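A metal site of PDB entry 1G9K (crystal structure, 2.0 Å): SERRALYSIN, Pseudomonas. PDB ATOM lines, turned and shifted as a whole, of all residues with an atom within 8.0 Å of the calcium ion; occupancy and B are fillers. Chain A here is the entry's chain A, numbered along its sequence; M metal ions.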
ATOM      1  N   HIS A  48     -26.562  12.792 -23.591  1.00  0.00           N
ATOM      2  CA  HIS A  48     -25.999  11.472 -23.804  1.00  0.00           C
ATOM      3  C   HIS A  48     -26.906  10.688 -24.737  1.00  0.00           C
ATOM      4  O   HIS A  48     -28.130  10.884 -24.747  1.00  0.00           O
ATOM      5  CB  HIS A  48     -25.853  10.753 -22.469  1.00  0.00           C
ATOM      6  CG  HIS A  48     -24.872  11.401 -21.542  1.00  0.00           C
ATOM      7  ND1 HIS A  48     -25.019  11.380 -20.174  1.00  0.00           N
ATOM      8  CD2 HIS A  48     -23.729  12.077 -21.791  1.00  0.00           C
ATOM      9  CE1 HIS A  48     -24.007  12.022 -19.619  1.00  0.00           C
ATOM     10  NE2 HIS A  48     -23.209  12.449 -20.583  1.00  0.00           N
ATOM     11  N   ASP A  49     -26.313   9.815 -25.551  1.00  0.00           N
ATOM     12  CA  ASP A  49     -27.060   8.979 -26.477  1.00  0.00           C
ATOM     13  C   ASP A  49     -27.523   7.752 -25.701  1.00  0.00           C
ATOM     14  O   ASP A  49     -26.879   6.701 -25.730  1.00  0.00           O
ATOM     15  CB  ASP A  49     -26.166   8.563 -27.652  1.00  0.00           C
ATOM     16  CG  ASP A  49     -26.909   7.807 -28.729  1.00  0.00           C
ATOM     17  OD1 ASP A  49     -28.145   7.622 -28.601  1.00  0.00           O
ATOM     18  OD2 ASP A  49     -26.272   7.394 -29.725  1.00  0.00           O
ATOM     19  N   LEU A  50     -28.645   7.888 -24.995  1.00  0.00           N
ATOM     20  CA  LEU A  50     -29.178   6.813 -24.174  1.00  0.00           C
ATOM     21  C   LEU A  50     -29.545   5.553 -24.956  1.00  0.00           C
ATOM     22  O   LEU A  50     -29.293   4.441 -24.500  1.00  0.00           O
ATOM     23  CB  LEU A  50     -30.407   7.313 -23.409  1.00  0.00           C
ATOM     24  CG  LEU A  50     -30.198   8.585 -22.571  1.00  0.00           C
ATOM     25  CD1 LEU A  50     -31.512   8.991 -21.930  1.00  0.00           C
ATOM     26  CD2 LEU A  50     -29.137   8.354 -21.514  1.00  0.00           C
ATOM     27  N   ASN A  51     -30.136   5.729 -26.136  1.00  0.00           N
ATOM     28  CA  ASN A  51     -30.534   4.583 -26.963  1.00  0.00           C
ATOM     29  C   ASN A  51     -29.409   4.079 -27.864  1.00  0.00           C
ATOM     30  O   ASN A  51     -29.572   3.083 -28.575  1.00  0.00           O
ATOM     31  CB  ASN A  51     -31.770   4.931 -27.802  1.00  0.00           C
ATOM     32  CG  ASN A  51     -31.617   6.245 -28.549  1.00  0.00           C
ATOM     33  OD1 ASN A  51     -30.671   6.442 -29.308  1.00  0.00           O
ATOM     34  ND2 ASN A  51     -32.571   7.144 -28.346  1.00  0.00           N
ATOM     35  N   ASN A  52     -28.272   4.762 -27.837  1.00  0.00           N
ATOM     36  CA  ASN A  52     -27.117   4.381 -28.649  1.00  0.00           C
ATOM     37  C   ASN A  52     -27.430   4.214 -30.122  1.00  0.00           C
ATOM     38  O   ASN A  52     -27.175   3.163 -30.696  1.00  0.00           O
ATOM     39  CB  ASN A  52     -26.521   3.075 -28.115  1.00  0.00           C
ATOM     40  CG  ASN A  52     -26.221   3.130 -26.634  1.00  0.00           C
ATOM     41  OD1 ASN A  52     -25.403   3.939 -26.185  1.00  0.00           O
ATOM     42  ND2 ASN A  52     -26.884   2.278 -25.854  1.00  0.00           N
ATOM     43  N   ASP A  53     -27.993   5.248 -30.739  1.00  0.00           N
ATOM     44  CA  ASP A  53     -28.321   5.166 -32.153  1.00  0.00           C
ATOM     45  C   ASP A  53     -27.437   6.086 -32.985  1.00  0.00           C
ATOM     46  O   ASP A  53     -27.660   6.250 -34.183  1.00  0.00           O
ATOM     47  CB  ASP A  53     -29.796   5.517 -32.386  1.00  0.00           C
ATOM     48  CG  ASP A  53     -30.136   6.932 -32.006  1.00  0.00           C
ATOM     49  OD1 ASP A  53     -31.286   7.362 -32.269  1.00  0.00           O
ATOM     50  OD2 ASP A  53     -29.258   7.626 -31.433  1.00  0.00           O
ATOM     51  N   GLY A  54     -26.438   6.676 -32.342  1.00  0.00           N
ATOM     52  CA  GLY A  54     -25.511   7.560 -33.052  1.00  0.00           C
ATOM     53  C   GLY A  54     -25.956   8.995 -33.244  1.00  0.00           C
ATOM     54  O   GLY A  54     -25.268   9.779 -33.900  1.00  0.00           O
ATOM     55  N   VAL A  55     -27.096   9.344 -32.673  1.00  0.00           N
ATOM     56  CA  VAL A  55     -27.624  10.698 -32.787  1.00  0.00           C
ATOM     57  C   VAL A  55     -28.384  11.078 -31.510  1.00  0.00           C
ATOM     58  O   VAL A  55     -29.020  10.235 -30.886  1.00  0.00           O
ATOM     59  CB  VAL A  55     -28.582  10.807 -33.998  1.00  0.00           C
ATOM     60  CG1 VAL A  55     -29.720   9.812 -33.855  1.00  0.00           C
ATOM     61  CG2 VAL A  55     -29.126  12.223 -34.112  1.00  0.00           C
ATOM     62  N   ILE A  56     -28.308  12.347 -31.141  1.00  0.00           N
ATOM     63  CA  ILE A  56     -28.997  12.823 -29.956  1.00  0.00           C
ATOM     64  C   ILE A  56     -30.418  13.175 -30.395  1.00  0.00           C
ATOM     65  O   ILE A  56     -30.617  14.140 -31.127  1.00  0.00           O
ATOM     66  CB  ILE A  56     -28.300  14.089 -29.380  1.00  0.00           C
ATOM     67  CG1 ILE A  56     -26.840  13.777 -29.019  1.00  0.00           C
ATOM     68  CG2 ILE A  56     -29.061  14.604 -28.169  1.00  0.00           C
ATOM     69  CD1 ILE A  56     -26.651  12.681 -27.969  1.00  0.00           C
ATOM     70  N   ASN A  57     -31.396  12.368 -29.977  1.00  0.00           N
ATOM     71  CA  ASN A  57     -32.791  12.612 -30.350  1.00  0.00           C
ATOM     72  C   ASN A  57     -33.500  13.360 -29.242  1.00  0.00           C
ATOM     73  O   ASN A  57     -33.798  12.791 -28.192  1.00  0.00           O
ATOM     74  CB  ASN A  57     -33.533  11.294 -30.594  1.00  0.00           C
ATOM     75  CG  ASN A  57     -32.617  10.158 -30.959  1.00  0.00           C
ATOM     76  OD1 ASN A  57     -31.988   9.548 -30.095  1.00  0.00           O
ATOM     77  ND2 ASN A  57     -32.517   9.868 -32.250  1.00  0.00           N
ATOM     78  N   LEU A  58     -33.778  14.634 -29.466  1.00  0.00           N
ATOM     79  CA  LEU A  58     -34.448  15.465 -28.475  1.00  0.00           C
ATOM     80  C   LEU A  58     -35.848  15.884 -28.910  1.00  0.00           C
ATOM     81  O   LEU A  58     -36.114  16.067 -30.094  1.00  0.00           O
ATOM     82  CB  LEU A  58     -33.622  16.727 -28.214  1.00  0.00           C
ATOM     83  CG  LEU A  58     -32.188  16.541 -27.709  1.00  0.00           C
ATOM     84  CD1 LEU A  58     -31.460  17.876 -27.718  1.00  0.00           C
ATOM     85  CD2 LEU A  58     -32.226  15.961 -26.295  1.00  0.00           C
ATOM     86  N   LYS A 101     -25.020  16.144 -35.290  1.00  0.00           N
ATOM     87  CA  LYS A 101     -25.917  14.997 -35.206  1.00  0.00           C
ATOM     88  C   LYS A 101     -26.867  15.084 -34.016  1.00  0.00           C
ATOM     89  O   LYS A 101     -26.797  14.288 -33.088  1.00  0.00           O
ATOM     90  CB  LYS A 101     -25.112  13.691 -35.130  1.00  0.00           C
ATOM     91  CG  LYS A 101     -24.367  13.326 -36.405  1.00  0.00           C
ATOM     92  CD  LYS A 101     -23.488  12.109 -36.186  1.00  0.00           C
ATOM     93  CE  LYS A 101     -22.912  11.566 -37.478  1.00  0.00           C
ATOM     94  NZ  LYS A 101     -21.971  10.418 -37.232  1.00  0.00           N
ATOM     95  N   THR A 103     -31.128  15.961 -33.289  1.00  0.00           N
ATOM     96  CA  THR A 103     -32.413  16.204 -33.923  1.00  0.00           C
ATOM     97  C   THR A 103     -33.381  16.766 -32.886  1.00  0.00           C
ATOM     98  O   THR A 103     -33.285  16.443 -31.697  1.00  0.00           O
ATOM     99  CB  THR A 103     -33.035  14.922 -34.532  1.00  0.00           C
ATOM    100  OG1 THR A 103     -33.310  13.968 -33.504  1.00  0.00           O
ATOM    101  CG2 THR A 103     -32.090  14.322 -35.561  1.00  0.00           C
ATOM    102  N   ASP A 113     -36.675   9.169 -25.744  1.00  0.00           N
ATOM    103  CA  ASP A 113     -35.850  10.269 -26.236  1.00  0.00           C
ATOM    104  C   ASP A 113     -34.590  10.357 -25.398  1.00  0.00           C
ATOM    105  O   ASP A 113     -34.518   9.762 -24.327  1.00  0.00           O
ATOM    106  CB  ASP A 113     -36.588  11.613 -26.123  1.00  0.00           C
ATOM    107  CG  ASP A 113     -38.026  11.544 -26.590  1.00  0.00           C
ATOM    108  OD1 ASP A 113     -38.281  10.953 -27.665  1.00  0.00           O
ATOM    109  OD2 ASP A 113     -38.896  12.103 -25.878  1.00  0.00           O
ATOM    110  N   ASP A 114     -33.603  11.113 -25.878  1.00  0.00           N
ATOM    111  CA  ASP A 114     -32.368  11.279 -25.120  1.00  0.00           C
ATOM    112  C   ASP A 114     -32.519  12.424 -24.128  1.00  0.00           C
ATOM    113  O   ASP A 114     -31.767  12.538 -23.165  1.00  0.00           O
ATOM    114  CB  ASP A 114     -31.199  11.568 -26.058  1.00  0.00           C
ATOM    115  CG  ASP A 114     -30.812  10.354 -26.887  1.00  0.00           C
ATOM    116  OD1 ASP A 114     -30.816   9.239 -26.327  1.00  0.00           O
ATOM    117  OD2 ASP A 114     -30.490  10.522 -28.079  1.00  0.00           O
ATOM    118  N   GLY A 115     -33.517  13.276 -24.376  1.00  0.00           N
ATOM    119  CA  GLY A 115     -33.778  14.412 -23.514  1.00  0.00           C
ATOM    120  C   GLY A 115     -34.976  15.201 -24.010  1.00  0.00           C
ATOM    121  O   GLY A 115     -35.458  14.978 -25.113  1.00  0.00           O
HETATM  122 CA    CA M   1     -29.970   8.717 -29.439  1.00  0.00          CA
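The nearest printed residue that does not touch the calcium ion is Ile 56 (4.3 Å).
The calcium ion is bound by OD1 of Asn 57 (2.3 Å). The calcium ion is bound by OD1 of Asp 49 (2.3 Å). O of Val 55 is bound to the calcium ion (2.3 Å). The calcium ion is bound by the side-chain carboxylate (OD2) of Asp 114 (2.3 Å). The calcium ion is bound by OD2 of Asp 53 (2.4 Å). OD1 of Asn 51 binds the calcium ion, at 2.4 Å. The calcium ion has six donor atoms within binding distance.
O of Asp 49 sits close to OD1 of Asn 52. OD2 of Asp 49 is in hydrogen-bond range of N of Gly 54. N of Leu 50 lies within hydrogen-bond range of OD1 of Asp 114 (2.9 Å).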
